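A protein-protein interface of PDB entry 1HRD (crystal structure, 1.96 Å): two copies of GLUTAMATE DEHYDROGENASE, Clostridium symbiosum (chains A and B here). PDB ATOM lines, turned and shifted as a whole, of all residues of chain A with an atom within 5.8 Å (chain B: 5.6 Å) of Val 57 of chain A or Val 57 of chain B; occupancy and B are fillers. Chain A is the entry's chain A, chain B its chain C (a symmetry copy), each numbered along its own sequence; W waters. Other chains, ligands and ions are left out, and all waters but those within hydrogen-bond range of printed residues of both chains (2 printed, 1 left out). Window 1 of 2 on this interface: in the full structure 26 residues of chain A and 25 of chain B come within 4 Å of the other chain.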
ATOM      1  N   PRO A  54     -14.550  34.951  -0.457  1.00  0.00           N
ATOM      2  CA  PRO A  54     -14.774  34.128  -1.619  1.00  0.00           C
ATOM      3  C   PRO A  54     -15.789  33.044  -1.321  1.00  0.00           C
ATOM      4  O   PRO A  54     -15.914  32.590  -0.177  1.00  0.00           O
ATOM      5  CB  PRO A  54     -13.427  33.452  -1.892  1.00  0.00           C
ATOM      6  CG  PRO A  54     -12.449  33.892  -0.817  1.00  0.00           C
ATOM      7  CD  PRO A  54     -13.187  34.815   0.122  1.00  0.00           C
ATOM      8  N   GLU A  55     -16.517  32.588  -2.328  1.00  0.00           N
ATOM      9  CA  GLU A  55     -17.472  31.503  -2.141  1.00  0.00           C
ATOM     10  C   GLU A  55     -16.783  30.231  -1.642  1.00  0.00           C
ATOM     11  O   GLU A  55     -17.206  29.577  -0.689  1.00  0.00           O
ATOM     12  CB  GLU A  55     -18.246  31.271  -3.459  1.00  0.00           C
ATOM     13  CG  GLU A  55     -19.195  32.457  -3.725  1.00  0.00           C
ATOM     14  CD  GLU A  55     -19.961  32.480  -5.032  1.00  0.00           C
ATOM     15  OE1 GLU A  55     -20.004  31.351  -5.697  1.00  0.00           O
ATOM     16  OE2 GLU A  55     -20.546  33.485  -5.408  1.00  0.00           O
ATOM     17  N   ARG A  56     -15.695  29.910  -2.329  1.00  0.00           N
ATOM     18  CA  ARG A  56     -14.910  28.718  -2.104  1.00  0.00           C
ATOM     19  C   ARG A  56     -13.434  28.914  -2.404  1.00  0.00           C
ATOM     20  O   ARG A  56     -13.062  29.527  -3.409  1.00  0.00           O
ATOM     21  CB  ARG A  56     -15.433  27.688  -3.111  1.00  0.00           C
ATOM     22  CG  ARG A  56     -15.123  26.232  -2.810  1.00  0.00           C
ATOM     23  CD  ARG A  56     -15.757  25.297  -3.834  1.00  0.00           C
ATOM     24  NE  ARG A  56     -17.219  25.299  -3.761  1.00  0.00           N
ATOM     25  CZ  ARG A  56     -18.038  25.847  -4.652  1.00  0.00           C
ATOM     26  NH1 ARG A  56     -17.593  26.455  -5.754  1.00  0.00           N
ATOM     27  NH2 ARG A  56     -19.347  25.803  -4.426  1.00  0.00           N
ATOM     28  N   VAL A  57     -12.614  28.340  -1.529  1.00  0.00           N
ATOM     29  CA  VAL A  57     -11.172  28.315  -1.641  1.00  0.00           C
ATOM     30  C   VAL A  57     -10.741  26.866  -1.558  1.00  0.00           C
ATOM     31  O   VAL A  57     -11.201  26.144  -0.671  1.00  0.00           O
ATOM     32  CB  VAL A  57     -10.480  29.012  -0.479  1.00  0.00           C
ATOM     33  CG1 VAL A  57      -8.967  28.831  -0.602  1.00  0.00           C
ATOM     34  CG2 VAL A  57     -10.854  30.488  -0.438  1.00  0.00           C
ATOM     35  N   ILE A  58      -9.855  26.470  -2.464  1.00  0.00           N
ATOM     36  CA  ILE A  58      -9.274  25.133  -2.520  1.00  0.00           C
ATOM     37  C   ILE A  58      -7.753  25.229  -2.560  1.00  0.00           C
ATOM     38  O   ILE A  58      -7.175  25.939  -3.386  1.00  0.00           O
ATOM     39  CB  ILE A  58      -9.745  24.306  -3.718  1.00  0.00           C
ATOM     40  CG1 ILE A  58     -11.259  24.101  -3.676  1.00  0.00           C
ATOM     41  CG2 ILE A  58      -9.044  22.951  -3.769  1.00  0.00           C
ATOM     42  CD1 ILE A  58     -11.975  24.798  -4.818  1.00  0.00           C
ATOM     43  N   GLU A  59      -7.090  24.505  -1.666  1.00  0.00           N
ATOM     44  CA  GLU A  59      -5.641  24.394  -1.683  1.00  0.00           C
ATOM     45  C   GLU A  59      -5.372  22.910  -1.698  1.00  0.00           C
ATOM     46  O   GLU A  59      -6.134  22.149  -1.102  1.00  0.00           O
ATOM     47  CB  GLU A  59      -4.881  24.992  -0.505  1.00  0.00           C
ATOM     48  CG  GLU A  59      -5.200  26.453  -0.276  1.00  0.00           C
ATOM     49  CD  GLU A  59      -4.377  26.994   0.840  1.00  0.00           C
ATOM     50  OE1 GLU A  59      -3.421  26.200   1.216  1.00  0.00           O
ATOM     51  OE2 GLU A  59      -4.564  28.068   1.342  1.00  0.00           O
ATOM     52  N   PHE A  60      -4.326  22.498  -2.374  1.00  0.00           N
ATOM     53  CA  PHE A  60      -4.063  21.073  -2.414  1.00  0.00           C
ATOM     54  C   PHE A  60      -2.597  20.787  -2.635  1.00  0.00           C
ATOM     55  O   PHE A  60      -1.887  21.619  -3.190  1.00  0.00           O
ATOM     56  CB  PHE A  60      -4.874  20.372  -3.523  1.00  0.00           C
ATOM     57  CG  PHE A  60      -4.805  21.039  -4.878  1.00  0.00           C
ATOM     58  CD1 PHE A  60      -5.694  22.071  -5.184  1.00  0.00           C
ATOM     59  CD2 PHE A  60      -3.887  20.643  -5.852  1.00  0.00           C
ATOM     60  CE1 PHE A  60      -5.677  22.710  -6.423  1.00  0.00           C
ATOM     61  CE2 PHE A  60      -3.861  21.259  -7.104  1.00  0.00           C
ATOM     62  CZ  PHE A  60      -4.748  22.302  -7.381  1.00  0.00           C
ATOM     63  N   ARG A  78      -6.899  27.435  -5.832  1.00  0.00           N
ATOM     64  CA  ARG A  78      -7.967  27.851  -6.730  1.00  0.00           C
ATOM     65  C   ARG A  78      -8.966  28.636  -5.909  1.00  0.00           C
ATOM     66  O   ARG A  78      -9.609  28.079  -5.025  1.00  0.00           O
ATOM     67  CB  ARG A  78      -8.603  26.793  -7.635  1.00  0.00           C
ATOM     68  CG  ARG A  78      -9.596  27.387  -8.632  1.00  0.00           C
ATOM     69  CD  ARG A  78      -8.947  28.199  -9.762  1.00  0.00           C
ATOM     70  NE  ARG A  78      -9.855  28.634 -10.840  1.00  0.00           N
ATOM     71  CZ  ARG A  78      -9.475  29.452 -11.819  1.00  0.00           C
ATOM     72  NH1 ARG A  78      -8.232  29.950 -11.867  1.00  0.00           N
ATOM     73  NH2 ARG A  78     -10.352  29.801 -12.772  1.00  0.00           N
ATOM     74  N   VAL A  79      -9.065  29.942  -6.130  1.00  0.00           N
ATOM     75  CA  VAL A  79      -9.999  30.757  -5.376  1.00  0.00           C
ATOM     76  C   VAL A  79     -11.197  31.058  -6.256  1.00  0.00           C
ATOM     77  O   VAL A  79     -11.047  31.781  -7.236  1.00  0.00           O
ATOM     78  CB  VAL A  79      -9.327  32.045  -4.905  1.00  0.00           C
ATOM     79  CG1 VAL A  79     -10.336  33.036  -4.309  1.00  0.00           C
ATOM     80  CG2 VAL A  79      -8.242  31.721  -3.888  1.00  0.00           C
ATOM     81  N   GLN A  80     -12.348  30.475  -5.945  1.00  0.00           N
ATOM     82  CA  GLN A  80     -13.572  30.699  -6.697  1.00  0.00           C
ATOM     83  C   GLN A  80     -14.303  31.777  -5.923  1.00  0.00           C
ATOM     84  O   GLN A  80     -15.075  31.491  -5.007  1.00  0.00           O
ATOM     85  CB  GLN A  80     -14.333  29.362  -6.828  1.00  0.00           C
ATOM     86  CG  GLN A  80     -13.431  28.258  -7.399  1.00  0.00           C
ATOM     87  CD  GLN A  80     -14.139  26.936  -7.624  1.00  0.00           C
ATOM     88  OE1 GLN A  80     -14.998  26.536  -6.817  1.00  0.00           O
ATOM     89  NE2 GLN A  80     -13.790  26.257  -8.723  1.00  0.00           N
ATOM     90  N   LEU A 100      -1.876  32.557  -0.694  1.00  0.00           N
ATOM     91  CA  LEU A 100      -3.280  32.875  -0.649  1.00  0.00           C
ATOM     92  C   LEU A 100      -3.669  34.338  -0.854  1.00  0.00           C
ATOM     93  O   LEU A 100      -4.603  34.623  -1.598  1.00  0.00           O
ATOM     94  CB  LEU A 100      -3.986  32.207   0.540  1.00  0.00           C
ATOM     95  CG  LEU A 100      -5.501  32.353   0.496  1.00  0.00           C
ATOM     96  CD1 LEU A 100      -6.123  31.493  -0.604  1.00  0.00           C
ATOM     97  CD2 LEU A 100      -6.096  32.019   1.858  1.00  0.00           C
ATOM     98  N   LYS A 104      -6.140  35.687  -3.500  1.00  0.00           N
ATOM     99  CA  LYS A 104      -7.348  36.403  -3.154  1.00  0.00           C
ATOM    100  C   LYS A 104      -7.417  37.783  -3.774  1.00  0.00           C
ATOM    101  O   LYS A 104      -8.455  38.218  -4.261  1.00  0.00           O
ATOM    102  CB  LYS A 104      -7.524  36.561  -1.653  1.00  0.00           C
ATOM    103  CG  LYS A 104      -7.953  35.284  -0.936  1.00  0.00           C
ATOM    104  CD  LYS A 104      -8.002  35.426   0.582  1.00  0.00           C
ATOM    105  CE  LYS A 104      -9.160  36.283   1.072  1.00  0.00           C
ATOM    106  NZ  LYS A 104      -9.261  36.333   2.539  1.00  0.00           N
ATOM    107  N   PRO B  54      -1.290  19.362   3.671  1.00  0.00           N
ATOM    108  CA  PRO B  54      -2.558  18.666   3.613  1.00  0.00           C
ATOM    109  C   PRO B  54      -2.892  18.258   2.200  1.00  0.00           C
ATOM    110  O   PRO B  54      -2.559  18.958   1.243  1.00  0.00           O
ATOM    111  CB  PRO B  54      -3.630  19.651   4.092  1.00  0.00           C
ATOM    112  CG  PRO B  54      -2.919  20.913   4.533  1.00  0.00           C
ATOM    113  CD  PRO B  54      -1.455  20.760   4.146  1.00  0.00           C
ATOM    114  N   GLU B  55      -3.575  17.130   2.063  1.00  0.00           N
ATOM    115  CA  GLU B  55      -3.944  16.721   0.736  1.00  0.00           C
ATOM    116  C   GLU B  55      -4.883  17.744   0.106  1.00  0.00           C
ATOM    117  O   GLU B  55      -4.806  18.029  -1.078  1.00  0.00           O
ATOM    118  CB  GLU B  55      -4.596  15.325   0.707  1.00  0.00           C
ATOM    119  CG  GLU B  55      -3.570  14.205   0.989  1.00  0.00           C
ATOM    120  CD  GLU B  55      -4.141  12.847   1.296  1.00  0.00           C
ATOM    121  OE1 GLU B  55      -5.315  12.611   0.792  1.00  0.00           O
ATOM    122  OE2 GLU B  55      -3.492  12.006   1.910  1.00  0.00           O
ATOM    123  N   ARG B  56      -5.780  18.287   0.907  1.00  0.00           N
ATOM    124  CA  ARG B  56      -6.746  19.218   0.370  1.00  0.00           C
ATOM    125  C   ARG B  56      -7.269  20.154   1.450  1.00  0.00           C
ATOM    126  O   ARG B  56      -7.540  19.700   2.557  1.00  0.00           O
ATOM    127  CB  ARG B  56      -7.872  18.363  -0.197  1.00  0.00           C
ATOM    128  CG  ARG B  56      -8.910  19.058  -1.054  1.00  0.00           C
ATOM    129  CD  ARG B  56     -10.064  18.150  -1.450  1.00  0.00           C
ATOM    130  NE  ARG B  56      -9.654  17.089  -2.366  1.00  0.00           N
ATOM    131  CZ  ARG B  56      -9.502  15.810  -2.035  1.00  0.00           C
ATOM    132  NH1 ARG B  56      -9.719  15.355  -0.796  1.00  0.00           N
ATOM    133  NH2 ARG B  56      -9.119  14.954  -2.983  1.00  0.00           N
ATOM    134  N   VAL B  57      -7.383  21.455   1.138  1.00  0.00           N
ATOM    135  CA  VAL B  57      -7.939  22.470   2.029  1.00  0.00           C
ATOM    136  C   VAL B  57      -9.139  23.099   1.343  1.00  0.00           C
ATOM    137  O   VAL B  57      -9.085  23.418   0.155  1.00  0.00           O
ATOM    138  CB  VAL B  57      -6.965  23.552   2.504  1.00  0.00           C
ATOM    139  CG1 VAL B  57      -7.687  24.575   3.376  1.00  0.00           C
ATOM    140  CG2 VAL B  57      -5.813  22.919   3.274  1.00  0.00           C
ATOM    141  N   ILE B  58     -10.213  23.240   2.107  1.00  0.00           N
ATOM    142  CA  ILE B  58     -11.458  23.858   1.664  1.00  0.00           C
ATOM    143  C   ILE B  58     -11.889  24.923   2.665  1.00  0.00           C
ATOM    144  O   ILE B  58     -11.993  24.676   3.869  1.00  0.00           O
ATOM    145  CB  ILE B  58     -12.622  22.889   1.392  1.00  0.00           C
ATOM    146  CG1 ILE B  58     -12.285  21.800   0.370  1.00  0.00           C
ATOM    147  CG2 ILE B  58     -13.864  23.664   0.952  1.00  0.00           C
ATOM    148  CD1 ILE B  58     -12.206  20.418   1.012  1.00  0.00           C
ATOM    149  N   GLU B  59     -12.108  26.131   2.145  1.00  0.00           N
ATOM    150  CA  GLU B  59     -12.640  27.270   2.887  1.00  0.00           C
ATOM    151  C   GLU B  59     -13.864  27.734   2.113  1.00  0.00           C
ATOM    152  O   GLU B  59     -13.900  27.652   0.890  1.00  0.00           O
ATOM    153  CB  GLU B  59     -11.715  28.464   3.194  1.00  0.00           C
ATOM    154  CG  GLU B  59     -10.272  28.099   3.549  1.00  0.00           C
ATOM    155  CD  GLU B  59      -9.432  29.263   4.014  1.00  0.00           C
ATOM    156  OE1 GLU B  59     -10.003  30.416   3.862  1.00  0.00           O
ATOM    157  OE2 GLU B  59      -8.343  29.125   4.515  1.00  0.00           O
ATOM    158  N   PHE B  60     -14.880  28.211   2.815  1.00  0.00           N
ATOM    159  CA  PHE B  60     -16.067  28.673   2.124  1.00  0.00           C
ATOM    160  C   PHE B  60     -16.857  29.681   2.932  1.00  0.00           C
ATOM    161  O   PHE B  60     -16.768  29.742   4.158  1.00  0.00           O
ATOM    162  CB  PHE B  60     -16.965  27.509   1.683  1.00  0.00           C
ATOM    163  CG  PHE B  60     -17.297  26.574   2.816  1.00  0.00           C
ATOM    164  CD1 PHE B  60     -16.467  25.498   3.130  1.00  0.00           C
ATOM    165  CD2 PHE B  60     -18.466  26.748   3.556  1.00  0.00           C
ATOM    166  CE1 PHE B  60     -16.765  24.616   4.169  1.00  0.00           C
ATOM    167  CE2 PHE B  60     -18.787  25.877   4.598  1.00  0.00           C
ATOM    168  CZ  PHE B  60     -17.942  24.807   4.898  1.00  0.00           C
ATOM    169  N   ARG B  78     -12.492  23.104   6.157  1.00  0.00           N
ATOM    170  CA  ARG B  78     -12.433  21.655   6.222  1.00  0.00           C
ATOM    171  C   ARG B  78     -11.053  21.278   5.743  1.00  0.00           C
ATOM    172  O   ARG B  78     -10.744  21.435   4.570  1.00  0.00           O
ATOM    173  CB  ARG B  78     -13.499  20.803   5.530  1.00  0.00           C
ATOM    174  CG  ARG B  78     -13.320  19.301   5.835  1.00  0.00           C
ATOM    175  CD  ARG B  78     -13.558  18.918   7.309  1.00  0.00           C
ATOM    176  NE  ARG B  78     -13.560  17.481   7.639  1.00  0.00           N
ATOM    177  CZ  ARG B  78     -13.616  16.984   8.882  1.00  0.00           C
ATOM    178  NH1 ARG B  78     -13.667  17.760   9.965  1.00  0.00           N
ATOM    179  NH2 ARG B  78     -13.604  15.660   9.055  1.00  0.00           N
ATOM    180  N   VAL B  79     -10.199  20.829   6.644  1.00  0.00           N
ATOM    181  CA  VAL B  79      -8.858  20.480   6.240  1.00  0.00           C
ATOM    182  C   VAL B  79      -8.684  18.964   6.160  1.00  0.00           C
ATOM    183  O   VAL B  79      -8.678  18.303   7.198  1.00  0.00           O
ATOM    184  CB  VAL B  79      -7.823  21.064   7.197  1.00  0.00           C
ATOM    185  CG1 VAL B  79      -6.432  20.498   6.872  1.00  0.00           C
ATOM    186  CG2 VAL B  79      -7.821  22.601   7.193  1.00  0.00           C
ATOM    187  N   GLN B  80      -8.569  18.413   4.948  1.00  0.00           N
ATOM    188  CA  GLN B  80      -8.402  16.986   4.724  1.00  0.00           C
ATOM    189  C   GLN B  80      -6.912  16.691   4.608  1.00  0.00           C
ATOM    190  O   GLN B  80      -6.341  16.689   3.521  1.00  0.00           O
ATOM    191  CB  GLN B  80      -9.214  16.555   3.486  1.00  0.00           C
ATOM    192  CG  GLN B  80     -10.677  17.006   3.609  1.00  0.00           C
ATOM    193  CD  GLN B  80     -11.586  16.582   2.465  1.00  0.00           C
ATOM    194  OE1 GLN B  80     -11.174  16.551   1.298  1.00  0.00           O
ATOM    195  NE2 GLN B  80     -12.835  16.247   2.786  1.00  0.00           N
ATOM    196  N   LEU B 100      -7.050  29.050   9.772  1.00  0.00           N
ATOM    197  CA  LEU B 100      -6.387  27.955   9.112  1.00  0.00           C
ATOM    198  C   LEU B 100      -5.265  27.279   9.900  1.00  0.00           C
ATOM    199  O   LEU B 100      -5.140  26.057   9.870  1.00  0.00           O
ATOM    200  CB  LEU B 100      -5.990  28.283   7.666  1.00  0.00           C
ATOM    201  CG  LEU B 100      -5.547  27.063   6.865  1.00  0.00           C
ATOM    202  CD1 LEU B 100      -6.708  26.102   6.660  1.00  0.00           C
ATOM    203  CD2 LEU B 100      -4.980  27.500   5.518  1.00  0.00           C
ATOM    204  N   LYS B 104      -5.046  23.495  10.772  1.00  0.00           N
ATOM    205  CA  LYS B 104      -3.939  22.708  10.273  1.00  0.00           C
ATOM    206  C   LYS B 104      -3.239  21.921  11.357  1.00  0.00           C
ATOM    207  O   LYS B 104      -2.991  20.724  11.238  1.00  0.00           O
ATOM    208  CB  LYS B 104      -2.939  23.568   9.526  1.00  0.00           C
ATOM    209  CG  LYS B 104      -3.370  23.700   8.080  1.00  0.00           C
ATOM    210  CD  LYS B 104      -2.524  24.690   7.306  1.00  0.00           C
ATOM    211  CE  LYS B 104      -1.135  24.155   7.018  1.00  0.00           C
ATOM    212  NZ  LYS B 104      -0.210  25.184   6.531  1.00  0.00           N
HETATM  213  O   HOH W   1      -2.971  21.748   0.581  1.00  0.00           O
HETATM  214  O   HOH W   2     -14.078  31.092   1.621  1.00  0.00           O
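Arg 56 of chain A touches Glu 59 of chain B, and with the chains exchanged Glu 59 of chain A touches Arg 56 of chain B.
Val 57 of chain A touches its own counterpart, Val 57 of chain B.
Val 57 of chain A touches Ile 58 of chain B, and with the chains exchanged Ile 58 of chain A touches Val 57 of chain B.
Val 57 of chain A touches Glu 59 of chain B, and with the chains exchanged Glu 59 of chain A touches Val 57 of chain B.
Of the 9 pairs that touch across the chains among the printed residues, 9 have their exchanged pair printed and touching as well.
Of the 12 printed residues of chain B, 6 touch a printed residue of chain A.
Of the 12 printed residues of chain A, 6 touch a printed residue of chain B.
Hydrophobic or aromatic side chains of chain A that line the printed part of chain B: Val 57, Ile 58 and Phe 60.
Among the printed residues, 9 pairs touch across the chains.
Among the printed residues, no Asp or Glu carboxylate lies within 4 Å of a Lys or Arg side-chain nitrogen of the other chain.
The backbone carbonyl oxygen of Gln 80 of chain A sits at hydrogen-bond distance from the backbone NH of Glu 55 of chain A, 3.2 Å away.
The backbone carbonyl oxygen (O) of Arg 56 of chain A sits at hydrogen-bond distance from the backbone NH (N) of Gln 80 of chain A, at 2.8 Å.
The backbone carbonyl oxygen (O) of Ile 58 of chain A sits at hydrogen-bond distance from the backbone NH (N) of Arg 78 of chain A.
The backbone carbonyl oxygen (O) of Gln 80 of chain B is in hydrogen-bond range of the backbone NH (N) of Glu 55 of chain B, 3.2 Å away.
The side-chain amide oxygen (OE1) of Gln 80 of chain B is in hydrogen-bond range of the guanidinium group (NH1) of Arg 56 of chain B.
O of Ile 58 of chain B lies within hydrogen-bond range of N of Arg 78 of chain B, at 2.8 Å.
Glu 55 of chain A touches Phe 60 of chain B.
Arg 56 of chain A touches Glu 59 of chain B.
Val 57 of chain B touches Val 57 of chain A (O to O, 3.5 Å).
Val 57 of chain A touches Ile 58 of chain B (O to CA, 3.3 Å).
O of Val 57 of chain B touches CA of Ile 58 of chain A (3.2 Å).
Arg 56 of chain B touches Glu 59 of chain A.
Phe 60 of chain A touches Glu 55 of chain B (CB to O, 3.4 Å).
Water W1 lies within hydrogen-bond range of the backbone carbonyl oxygen (O) of Pro 54 of chain B (2.9 Å) and the backbone NH (N) of Phe 60 of chain A (3.3 Å).
Water W2 bridges O of Pro 54 of chain A and N of Phe 60 of chain B.
Of chain B, only Val 57, Ile 58 and Glu 59 come within 4 Å of Val 57 of chain A.
Val 57 of chain B touches just these residues of chain A: Val 57 (3.5 Å), Ile 58 (3.2 Å) and Glu 59 (2.7 Å).
Of the printed residues of chain A, Glu 55 of chain B touches Phe 60 (3.4 Å).
Of the printed residues of chain A, Phe 60 of chain B touches Glu 55.
Val 79 of chain A touches none of the printed residues of chain B.
Leu 100 of chain B touches none of the printed residues of chain A.
The nearest residue of chain B that does not touch Val 57 of chain A is Phe 60 of chain B (4.9 Å).
The nearest residue of chain A that does not touch Val 57 of chain B is Phe 60 of chain A (4.8 Å).
The backbone carbonyl oxygen of Glu 59 of chain B sits at hydrogen-bond distance from the backbone NH of Val 57 of chain A (2.8 Å).
The backbone NH (N) of Val 57 of chain B lies within hydrogen-bond range of the backbone carbonyl oxygen (O) of Glu 59 of chain A.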
